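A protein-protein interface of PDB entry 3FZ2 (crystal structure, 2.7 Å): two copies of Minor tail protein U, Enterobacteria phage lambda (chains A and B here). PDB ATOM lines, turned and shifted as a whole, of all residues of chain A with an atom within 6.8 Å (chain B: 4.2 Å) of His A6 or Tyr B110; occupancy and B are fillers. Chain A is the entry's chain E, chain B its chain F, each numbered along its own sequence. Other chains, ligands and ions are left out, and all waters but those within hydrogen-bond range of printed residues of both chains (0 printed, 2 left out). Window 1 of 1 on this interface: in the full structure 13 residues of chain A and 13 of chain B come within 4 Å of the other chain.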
ATOM      1  N   HIS A   3      25.612  -7.878  -4.588  1.00  0.00           N
ATOM      2  CA  HIS A   3      24.385  -8.574  -4.185  1.00  0.00           C
ATOM      3  C   HIS A   3      23.190  -8.136  -5.034  1.00  0.00           C
ATOM      4  O   HIS A   3      23.213  -7.069  -5.650  1.00  0.00           O
ATOM      5  CB  HIS A   3      24.076  -8.297  -2.712  1.00  0.00           C
ATOM      6  CG  HIS A   3      24.452  -9.415  -1.790  1.00  0.00           C
ATOM      7  ND1 HIS A   3      24.442  -9.283  -0.418  1.00  0.00           N
ATOM      8  CD2 HIS A   3      24.838 -10.688  -2.041  1.00  0.00           C
ATOM      9  CE1 HIS A   3      24.809 -10.424   0.136  1.00  0.00           C
ATOM     10  NE2 HIS A   3      25.054 -11.293  -0.827  1.00  0.00           N
ATOM     11  N   MET A   4      22.146  -8.961  -5.059  1.00  0.00           N
ATOM     12  CA  MET A   4      20.946  -8.658  -5.834  1.00  0.00           C
ATOM     13  C   MET A   4      20.207  -7.472  -5.212  1.00  0.00           C
ATOM     14  O   MET A   4      20.231  -7.297  -3.995  1.00  0.00           O
ATOM     15  CB  MET A   4      20.023  -9.871  -5.866  1.00  0.00           C
ATOM     16  CG  MET A   4      19.136  -9.927  -7.087  1.00  0.00           C
ATOM     17  SD  MET A   4      17.476 -10.813  -6.714  1.00  0.00           S
ATOM     18  CE  MET A   4      16.281  -9.378  -7.177  1.00  0.00           C
ATOM     19  N   LYS A   5      19.544  -6.670  -6.044  1.00  0.00           N
ATOM     20  CA  LYS A   5      18.829  -5.495  -5.554  1.00  0.00           C
ATOM     21  C   LYS A   5      17.868  -5.790  -4.398  1.00  0.00           C
ATOM     22  O   LYS A   5      17.898  -5.102  -3.376  1.00  0.00           O
ATOM     23  CB  LYS A   5      18.071  -4.814  -6.699  1.00  0.00           C
ATOM     24  CG  LYS A   5      17.828  -3.318  -6.477  1.00  0.00           C
ATOM     25  CD  LYS A   5      19.156  -2.590  -6.227  1.00  0.00           C
ATOM     26  CE  LYS A   5      19.059  -1.083  -6.453  1.00  0.00           C
ATOM     27  NZ  LYS A   5      18.984  -0.694  -7.900  1.00  0.00           N
ATOM     28  N   HIS A   6      17.021  -6.807  -4.545  1.00  0.00           N
ATOM     29  CA  HIS A   6      16.079  -7.153  -3.482  1.00  0.00           C
ATOM     30  C   HIS A   6      16.750  -7.387  -2.144  1.00  0.00           C
ATOM     31  O   HIS A   6      16.211  -7.022  -1.102  1.00  0.00           O
ATOM     32  CB  HIS A   6      15.278  -8.388  -3.860  1.00  0.00           C
ATOM     33  CG  HIS A   6      14.315  -8.145  -4.972  1.00  0.00           C
ATOM     34  ND1 HIS A   6      13.347  -9.056  -5.334  1.00  0.00           N
ATOM     35  CD2 HIS A   6      14.153  -7.077  -5.785  1.00  0.00           C
ATOM     36  CE1 HIS A   6      12.626  -8.556  -6.322  1.00  0.00           C
ATOM     37  NE2 HIS A   6      13.095  -7.355  -6.613  1.00  0.00           N
ATOM     38  N   THR A   7      17.922  -8.011  -2.177  1.00  0.00           N
ATOM     39  CA  THR A   7      18.686  -8.285  -0.971  1.00  0.00           C
ATOM     40  C   THR A   7      19.187  -6.978  -0.360  1.00  0.00           C
ATOM     41  O   THR A   7      19.044  -6.732   0.847  1.00  0.00           O
ATOM     42  CB  THR A   7      19.888  -9.166  -1.292  1.00  0.00           C
ATOM     43  OG1 THR A   7      19.426 -10.461  -1.681  1.00  0.00           O
ATOM     44  CG2 THR A   7      20.791  -9.293  -0.091  1.00  0.00           C
ATOM     45  N   GLU A   8      19.779  -6.135  -1.195  1.00  0.00           N
ATOM     46  CA  GLU A   8      20.287  -4.871  -0.703  1.00  0.00           C
ATOM     47  C   GLU A   8      19.159  -4.033  -0.114  1.00  0.00           C
ATOM     48  O   GLU A   8      19.349  -3.395   0.914  1.00  0.00           O
ATOM     49  CB  GLU A   8      20.999  -4.130  -1.825  1.00  0.00           C
ATOM     50  CG  GLU A   8      21.966  -5.031  -2.551  1.00  0.00           C
ATOM     51  CD  GLU A   8      22.889  -4.289  -3.490  1.00  0.00           C
ATOM     52  OE1 GLU A   8      22.389  -3.526  -4.351  1.00  0.00           O
ATOM     53  OE2 GLU A   8      24.120  -4.483  -3.365  1.00  0.00           O
ATOM     54  N   LEU A   9      17.988  -4.060  -0.745  1.00  0.00           N
ATOM     55  CA  LEU A   9      16.843  -3.300  -0.265  1.00  0.00           C
ATOM     56  C   LEU A   9      16.412  -3.722   1.130  1.00  0.00           C
ATOM     57  O   LEU A   9      16.306  -2.886   2.031  1.00  0.00           O
ATOM     58  CB  LEU A   9      15.652  -3.447  -1.212  1.00  0.00           C
ATOM     59  CG  LEU A   9      15.779  -2.753  -2.565  1.00  0.00           C
ATOM     60  CD1 LEU A   9      14.575  -3.070  -3.418  1.00  0.00           C
ATOM     61  CD2 LEU A   9      15.932  -1.263  -2.352  1.00  0.00           C
ATOM     62  N   ARG A  10      16.148  -5.011   1.317  1.00  0.00           N
ATOM     63  CA  ARG A  10      15.735  -5.502   2.627  1.00  0.00           C
ATOM     64  C   ARG A  10      16.850  -5.298   3.654  1.00  0.00           C
ATOM     65  O   ARG A  10      16.589  -4.977   4.821  1.00  0.00           O
ATOM     66  CB  ARG A  10      15.393  -6.988   2.558  1.00  0.00           C
ATOM     67  CG  ARG A  10      14.259  -7.345   1.605  1.00  0.00           C
ATOM     68  CD  ARG A  10      13.875  -8.800   1.766  1.00  0.00           C
ATOM     69  NE  ARG A  10      14.975  -9.693   1.423  1.00  0.00           N
ATOM     70  CZ  ARG A  10      15.078 -10.331   0.263  1.00  0.00           C
ATOM     71  NH1 ARG A  10      14.143 -10.176  -0.663  1.00  0.00           N
ATOM     72  NH2 ARG A  10      16.110 -11.125   0.031  1.00  0.00           N
ATOM     73  N   ALA A  11      18.092  -5.485   3.210  1.00  0.00           N
ATOM     74  CA  ALA A  11      19.245  -5.345   4.088  1.00  0.00           C
ATOM     75  C   ALA A  11      19.364  -3.930   4.636  1.00  0.00           C
ATOM     76  O   ALA A  11      19.661  -3.736   5.812  1.00  0.00           O
ATOM     77  CB  ALA A  11      20.526  -5.742   3.346  1.00  0.00           C
ATOM     78  N   ASP A  28      14.240 -12.184   7.388  1.00  0.00           N
ATOM     79  CA  ASP A  28      14.484 -11.738   6.024  1.00  0.00           C
ATOM     80  C   ASP A  28      13.490 -12.542   5.197  1.00  0.00           C
ATOM     81  O   ASP A  28      13.780 -13.661   4.781  1.00  0.00           O
ATOM     82  CB  ASP A  28      15.919 -12.081   5.626  1.00  0.00           C
ATOM     83  CG  ASP A  28      16.262 -11.641   4.222  1.00  0.00           C
ATOM     84  OD1 ASP A  28      15.959 -10.486   3.858  1.00  0.00           O
ATOM     85  OD2 ASP A  28      16.854 -12.450   3.482  1.00  0.00           O
ATOM     86  N   LEU A  46       9.507  -8.364   0.589  1.00  0.00           N
ATOM     87  CA  LEU A  46       8.892  -7.812  -0.610  1.00  0.00           C
ATOM     88  C   LEU A  46       7.827  -8.730  -1.209  1.00  0.00           C
ATOM     89  O   LEU A  46       7.942  -9.949  -1.134  1.00  0.00           O
ATOM     90  CB  LEU A  46       9.954  -7.590  -1.678  1.00  0.00           C
ATOM     91  CG  LEU A  46      11.169  -6.732  -1.347  1.00  0.00           C
ATOM     92  CD1 LEU A  46      12.207  -6.914  -2.424  1.00  0.00           C
ATOM     93  CD2 LEU A  46      10.764  -5.273  -1.228  1.00  0.00           C
ATOM     94  N   THR A  47       6.792  -8.130  -1.794  1.00  0.00           N
ATOM     95  CA  THR A  47       5.738  -8.868  -2.490  1.00  0.00           C
ATOM     96  C   THR A  47       5.428  -8.090  -3.767  1.00  0.00           C
ATOM     97  O   THR A  47       5.719  -6.893  -3.855  1.00  0.00           O
ATOM     98  CB  THR A  47       4.400  -8.997  -1.693  1.00  0.00           C
ATOM     99  OG1 THR A  47       3.813  -7.699  -1.509  1.00  0.00           O
ATOM    100  CG2 THR A  47       4.625  -9.673  -0.345  1.00  0.00           C
ATOM    101  N   GLY A  48       4.863  -8.790  -4.752  1.00  0.00           N
ATOM    102  CA  GLY A  48       4.474  -8.183  -6.010  1.00  0.00           C
ATOM    103  C   GLY A  48       5.524  -7.637  -6.957  1.00  0.00           C
ATOM    104  O   GLY A  48       5.172  -6.990  -7.934  1.00  0.00           O
ATOM    105  N   ALA A  49       6.802  -7.889  -6.708  1.00  0.00           N
ATOM    106  CA  ALA A  49       7.849  -7.374  -7.587  1.00  0.00           C
ATOM    107  C   ALA A  49       7.534  -7.689  -9.031  1.00  0.00           C
ATOM    108  O   ALA A  49       7.303  -8.842  -9.389  1.00  0.00           O
ATOM    109  CB  ALA A  49       9.182  -7.971  -7.221  1.00  0.00           C
ATOM    110  N   GLU A  50       7.524  -6.660  -9.864  1.00  0.00           N
ATOM    111  CA  GLU A  50       7.241  -6.859 -11.270  1.00  0.00           C
ATOM    112  C   GLU A  50       7.792  -5.753 -12.155  1.00  0.00           C
ATOM    113  O   GLU A  50       7.793  -4.577 -11.783  1.00  0.00           O
ATOM    114  CB  GLU A  50       5.740  -6.995 -11.486  1.00  0.00           C
ATOM    115  CG  GLU A  50       4.936  -5.866 -10.920  1.00  0.00           C
ATOM    116  CD  GLU A  50       3.524  -5.863 -11.456  1.00  0.00           C
ATOM    117  OE1 GLU A  50       2.867  -6.924 -11.396  1.00  0.00           O
ATOM    118  OE2 GLU A  50       3.073  -4.803 -11.940  1.00  0.00           O
ATOM    119  N   TYR A  51       8.273  -6.163 -13.323  1.00  0.00           N
ATOM    120  CA  TYR A  51       8.840  -5.265 -14.315  1.00  0.00           C
ATOM    121  C   TYR A  51       7.789  -4.228 -14.721  1.00  0.00           C
ATOM    122  O   TYR A  51       6.643  -4.577 -14.988  1.00  0.00           O
ATOM    123  CB  TYR A  51       9.258  -6.083 -15.531  1.00  0.00           C
ATOM    124  CG  TYR A  51       9.780  -5.266 -16.674  1.00  0.00           C
ATOM    125  CD1 TYR A  51      11.035  -4.672 -16.616  1.00  0.00           C
ATOM    126  CD2 TYR A  51       9.015  -5.069 -17.812  1.00  0.00           C
ATOM    127  CE1 TYR A  51      11.514  -3.901 -17.669  1.00  0.00           C
ATOM    128  CE2 TYR A  51       9.482  -4.304 -18.864  1.00  0.00           C
ATOM    129  CZ  TYR A  51      10.729  -3.724 -18.787  1.00  0.00           C
ATOM    130  OH  TYR A  51      11.186  -2.964 -19.831  1.00  0.00           O
ATOM    131  N   TRP A  61      11.302  -1.503 -11.937  1.00  0.00           N
ATOM    132  CA  TRP A  61      10.517  -2.530 -11.275  1.00  0.00           C
ATOM    133  C   TRP A  61       9.691  -1.853 -10.197  1.00  0.00           C
ATOM    134  O   TRP A  61      10.045  -0.774  -9.721  1.00  0.00           O
ATOM    135  CB  TRP A  61      11.417  -3.581 -10.638  1.00  0.00           C
ATOM    136  CG  TRP A  61      11.862  -4.600 -11.603  1.00  0.00           C
ATOM    137  CD1 TRP A  61      12.683  -4.407 -12.669  1.00  0.00           C
ATOM    138  CD2 TRP A  61      11.475  -5.977 -11.632  1.00  0.00           C
ATOM    139  NE1 TRP A  61      12.833  -5.577 -13.369  1.00  0.00           N
ATOM    140  CE2 TRP A  61      12.103  -6.561 -12.756  1.00  0.00           C
ATOM    141  CE3 TRP A  61      10.659  -6.778 -10.817  1.00  0.00           C
ATOM    142  CZ2 TRP A  61      11.941  -7.913 -13.092  1.00  0.00           C
ATOM    143  CZ3 TRP A  61      10.499  -8.126 -11.150  1.00  0.00           C
ATOM    144  CH2 TRP A  61      11.139  -8.676 -12.280  1.00  0.00           C
ATOM    145  N   ALA A  63       7.491  -2.790  -6.508  1.00  0.00           N
ATOM    146  CA  ALA A  63       7.208  -3.855  -5.549  1.00  0.00           C
ATOM    147  C   ALA A  63       6.674  -3.295  -4.246  1.00  0.00           C
ATOM    148  O   ALA A  63       6.674  -2.094  -4.028  1.00  0.00           O
ATOM    149  CB  ALA A  63       8.465  -4.698  -5.287  1.00  0.00           C
ATOM    150  N   TYR A 132      12.184   0.783  -8.381  1.00  0.00           N
ATOM    151  CA  TYR A 132      13.636   0.695  -8.428  1.00  0.00           C
ATOM    152  C   TYR A 132      14.070   0.005  -9.708  1.00  0.00           C
ATOM    153  O   TYR A 132      13.245  -0.521 -10.454  1.00  0.00           O
ATOM    154  CB  TYR A 132      14.124  -0.110  -7.223  1.00  0.00           C
ATOM    155  CG  TYR A 132      13.444  -1.465  -7.120  1.00  0.00           C
ATOM    156  CD1 TYR A 132      14.098  -2.635  -7.515  1.00  0.00           C
ATOM    157  CD2 TYR A 132      12.125  -1.568  -6.680  1.00  0.00           C
ATOM    158  CE1 TYR A 132      13.452  -3.875  -7.474  1.00  0.00           C
ATOM    159  CE2 TYR A 132      11.469  -2.792  -6.641  1.00  0.00           C
ATOM    160  CZ  TYR A 132      12.134  -3.940  -7.038  1.00  0.00           C
ATOM    161  OH  TYR A 132      11.474  -5.143  -7.012  1.00  0.00           O
ATOM    162  N   MET A 134      16.727  -2.902 -11.433  1.00  0.00           N
ATOM    163  CA  MET A 134      17.447  -4.101 -11.031  1.00  0.00           C
ATOM    164  C   MET A 134      18.944  -3.903 -11.189  1.00  0.00           C
ATOM    165  O   MET A 134      19.339  -2.882 -11.806  1.00  0.00           O
ATOM    166  OXT MET A 134      19.696  -4.774 -10.692  1.00  0.00           O
ATOM    167  CB  MET A 134      16.991  -5.300 -11.857  1.00  0.00           C
ATOM    168  CG  MET A 134      15.704  -5.942 -11.359  1.00  0.00           C
ATOM    169  SD  MET A 134      15.882  -6.903  -9.672  1.00  0.00           S
ATOM    170  CE  MET A 134      14.056  -7.500  -9.501  1.00  0.00           C
ATOM    171  N   ASP B  81      17.732 -15.325  -3.283  1.00  0.00           N
ATOM    172  CA  ASP B  81      18.228 -14.278  -4.162  1.00  0.00           C
ATOM    173  C   ASP B  81      19.690 -14.508  -4.571  1.00  0.00           C
ATOM    174  O   ASP B  81      20.097 -14.166  -5.681  1.00  0.00           O
ATOM    175  CB  ASP B  81      18.122 -12.908  -3.482  1.00  0.00           C
ATOM    176  CG  ASP B  81      16.692 -12.442  -3.308  1.00  0.00           C
ATOM    177  OD1 ASP B  81      15.810 -12.897  -4.062  1.00  0.00           O
ATOM    178  OD2 ASP B  81      16.455 -11.595  -2.428  1.00  0.00           O
ATOM    179  N   MET B  84      19.878 -16.882  -7.502  1.00  0.00           N
ATOM    180  CA  MET B  84      19.422 -16.155  -8.669  1.00  0.00           C
ATOM    181  C   MET B  84      20.525 -15.273  -9.222  1.00  0.00           C
ATOM    182  O   MET B  84      20.785 -15.273 -10.420  1.00  0.00           O
ATOM    183  CB  MET B  84      18.223 -15.298  -8.297  1.00  0.00           C
ATOM    184  CG  MET B  84      16.922 -16.052  -8.317  1.00  0.00           C
ATOM    185  SD  MET B  84      16.327 -16.413 -10.130  1.00  0.00           S
ATOM    186  CE  MET B  84      14.687 -17.317  -9.681  1.00  0.00           C
ATOM    187  N   TYR B  89      20.514 -15.193 -13.339  1.00  0.00           N
ATOM    188  CA  TYR B  89      20.641 -13.937 -14.083  1.00  0.00           C
ATOM    189  C   TYR B  89      21.815 -13.898 -15.052  1.00  0.00           C
ATOM    190  O   TYR B  89      21.677 -13.426 -16.175  1.00  0.00           O
ATOM    191  CB  TYR B  89      20.759 -12.738 -13.142  1.00  0.00           C
ATOM    192  CG  TYR B  89      19.456 -12.284 -12.533  1.00  0.00           C
ATOM    193  CD1 TYR B  89      19.093 -12.684 -11.253  1.00  0.00           C
ATOM    194  CD2 TYR B  89      18.594 -11.441 -13.232  1.00  0.00           C
ATOM    195  CE1 TYR B  89      17.910 -12.258 -10.675  1.00  0.00           C
ATOM    196  CE2 TYR B  89      17.402 -11.012 -12.666  1.00  0.00           C
ATOM    197  CZ  TYR B  89      17.070 -11.424 -11.382  1.00  0.00           C
ATOM    198  OH  TYR B  89      15.909 -10.995 -10.787  1.00  0.00           O
ATOM    199  N   GLY B 109       8.057 -10.790 -13.692  1.00  0.00           N
ATOM    200  CA  GLY B 109       7.924 -10.718 -12.251  1.00  0.00           C
ATOM    201  C   GLY B 109       8.947 -11.537 -11.490  1.00  0.00           C
ATOM    202  O   GLY B 109       9.677 -12.350 -12.061  1.00  0.00           O
ATOM    203  N   TYR B 110       9.007 -11.301 -10.186  1.00  0.00           N
ATOM    204  CA  TYR B 110       9.917 -12.006  -9.293  1.00  0.00           C
ATOM    205  C   TYR B 110       9.128 -12.227  -8.001  1.00  0.00           C
ATOM    206  O   TYR B 110       8.935 -11.297  -7.207  1.00  0.00           O
ATOM    207  CB  TYR B 110      11.153 -11.161  -9.015  1.00  0.00           C
ATOM    208  CG  TYR B 110      12.267 -11.917  -8.332  1.00  0.00           C
ATOM    209  CD1 TYR B 110      13.332 -12.439  -9.071  1.00  0.00           C
ATOM    210  CD2 TYR B 110      12.270 -12.107  -6.946  1.00  0.00           C
ATOM    211  CE1 TYR B 110      14.382 -13.129  -8.451  1.00  0.00           C
ATOM    212  CE2 TYR B 110      13.307 -12.791  -6.318  1.00  0.00           C
ATOM    213  CZ  TYR B 110      14.364 -13.300  -7.077  1.00  0.00           C
ATOM    214  OH  TYR B 110      15.407 -13.964  -6.468  1.00  0.00           O
ATOM    215  N   ASP B 111       8.669 -13.462  -7.809  1.00  0.00           N
ATOM    216  CA  ASP B 111       7.861 -13.816  -6.654  1.00  0.00           C
ATOM    217  C   ASP B 111       8.520 -14.762  -5.672  1.00  0.00           C
ATOM    218  O   ASP B 111       9.349 -15.587  -6.050  1.00  0.00           O
ATOM    219  CB  ASP B 111       6.553 -14.439  -7.129  1.00  0.00           C
ATOM    220  CG  ASP B 111       5.726 -13.476  -7.941  1.00  0.00           C
ATOM    221  OD1 ASP B 111       5.204 -12.509  -7.340  1.00  0.00           O
ATOM    222  OD2 ASP B 111       5.609 -13.669  -9.176  1.00  0.00           O
ATOM    223  N   TYR B 112       8.145 -14.623  -4.404  1.00  0.00           N
ATOM    224  CA  TYR B 112       8.643 -15.493  -3.351  1.00  0.00           C
ATOM    225  C   TYR B 112       7.468 -16.411  -3.000  1.00  0.00           C
ATOM    226  O   TYR B 112       6.424 -15.953  -2.559  1.00  0.00           O
ATOM    227  CB  TYR B 112       9.091 -14.669  -2.142  1.00  0.00           C
ATOM    228  CG  TYR B 112      10.304 -13.803  -2.412  1.00  0.00           C
ATOM    229  CD1 TYR B 112      10.160 -12.471  -2.810  1.00  0.00           C
ATOM    230  CD2 TYR B 112      11.605 -14.332  -2.322  1.00  0.00           C
ATOM    231  CE1 TYR B 112      11.283 -11.681  -3.119  1.00  0.00           C
ATOM    232  CE2 TYR B 112      12.739 -13.548  -2.630  1.00  0.00           C
ATOM    233  CZ  TYR B 112      12.565 -12.231  -3.032  1.00  0.00           C
ATOM    234  OH  TYR B 112      13.650 -11.474  -3.394  1.00  0.00           O
ATOM    235  N   ALA B 124      11.849 -18.845  -5.127  1.00  0.00           N
ATOM    236  CA  ALA B 124      11.916 -17.581  -5.853  1.00  0.00           C
ATOM    237  C   ALA B 124      11.650 -17.910  -7.325  1.00  0.00           C
ATOM    238  O   ALA B 124      12.458 -18.551  -7.992  1.00  0.00           O
ATOM    239  CB  ALA B 124      13.283 -16.927  -5.682  1.00  0.00           C
ATOM    240  N   ASP B 125      10.500 -17.467  -7.818  1.00  0.00           N
ATOM    241  CA  ASP B 125      10.087 -17.732  -9.188  1.00  0.00           C
ATOM    242  C   ASP B 125      10.287 -16.517 -10.110  1.00  0.00           C
ATOM    243  O   ASP B 125       9.601 -15.499  -9.983  1.00  0.00           O
ATOM    244  CB  ASP B 125       8.621 -18.195  -9.159  1.00  0.00           C
ATOM    245  CG  ASP B 125       8.083 -18.559 -10.523  1.00  0.00           C
ATOM    246  OD1 ASP B 125       8.872 -18.869 -11.422  1.00  0.00           O
ATOM    247  OD2 ASP B 125       6.850 -18.552 -10.696  1.00  0.00           O
ATOM    248  N   LEU B 126      11.254 -16.631 -11.020  1.00  0.00           N
ATOM    249  CA  LEU B 126      11.564 -15.570 -11.977  1.00  0.00           C
ATOM    250  C   LEU B 126      10.778 -15.842 -13.263  1.00  0.00           C
ATOM    251  O   LEU B 126      10.892 -16.919 -13.840  1.00  0.00           O
ATOM    252  CB  LEU B 126      13.067 -15.555 -12.270  1.00  0.00           C
ATOM    253  CG  LEU B 126      13.581 -14.602 -13.361  1.00  0.00           C
ATOM    254  CD1 LEU B 126      13.158 -13.158 -13.036  1.00  0.00           C
ATOM    255  CD2 LEU B 126      15.101 -14.690 -13.463  1.00  0.00           C
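The side-chain carboxylate (OD2) of Asp B81 lies within hydrogen-bond range of the side-chain hydroxyl (OG1) of Thr A7 (3.3 Å). OH of Tyr B110 sits at hydrogen-bond distance from SD of Met A4 (3.8 Å). The side-chain hydroxyl of Tyr B112 lies within hydrogen-bond range of the guanidinium group of Arg A10, at 3.1 Å. The side-chain sulfur (SD) of Met A4 lies close to the side-chain carboxylate (OD1) of Asp B81 (3.8 Å). The guanidinium group of Arg A10 lies within salt-bridge range of the side-chain carboxylate of Asp B81, at 2.5 Å. The side-chain hydroxyl of Tyr B112 lies within hydrogen-bond range of a ring nitrogen (ND1) of His A6, 3.1 Å away. N of Tyr B110 sits at hydrogen-bond distance from O of Ala A49 (3.1 Å).
Printed residues of chain A that touch a printed residue of chain B: Met A4, His A6, Thr A7, Arg A10, Leu A46, Ala A49 and Trp A61. Hydrophobic or aromatic side chains of chain A within 4 Å of the printed part of chain B: Met A4, His A6, Ala A49 and Trp A61. Of the 10 printed residues of chain B, 5 touch a printed residue of chain A. Hydrophobic or aromatic side chains of chain B that line the printed part of chain A: Tyr B89, Tyr B110 and Tyr B112.
OH of Tyr B89 touches CE of Met A4, 3.97 Å away. His A6 touches Asp B81. His A6 touches Tyr B110. Leu A46 touches Tyr B112. Gly B109 touches Ala A49 (CA to O, 3.5 Å). Trp A61 touches Gly B109 (CH2 to C, 3.7 Å). CZ3 of Trp A61 touches N of Tyr B110 (3.6 Å).
No position is printed for both chains.
The guanidinium group (NE) of Arg A10 is in salt-bridge range of the side-chain carboxylate (OD1) of Asp A28, at 2.7 Å. The side-chain carboxylate (OD1) of Asp B81 sits at hydrogen-bond distance from the side-chain hydroxyl (OH) of Tyr B112 (2.7 Å). The backbone NH (N) of Tyr B89 is in hydrogen-bond range of the backbone carbonyl oxygen (O) of Met B84, 2.9 Å away. The side-chain hydroxyl (OH) of Tyr A132 lies within hydrogen-bond range of a ring nitrogen (NE2) of His A6, 2.8 Å away. The backbone NH of Trp A61 is in hydrogen-bond range of the backbone carbonyl oxygen of Tyr A132. The side-chain carboxylate (OD1) of Asp B81 is in hydrogen-bond range of the side-chain hydroxyl (OH) of Tyr B110, at 2.7 Å.
Of the printed residues of chain B, Met A4 touches Asp B81, Tyr B89 and Tyr B110. Of the printed residues of chain B, His A6 touches Asp B81, Tyr B110 and Tyr B112. Of the printed residues of chain A, Tyr B112 touches His A6, Arg A10 and Leu A46. The nearest printed residue of chain B that does not touch His A6 is Tyr B89 (6.1 Å). The nearest printed residue of chain B that does not touch Trp A61 is Leu B126 (5.0 Å).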
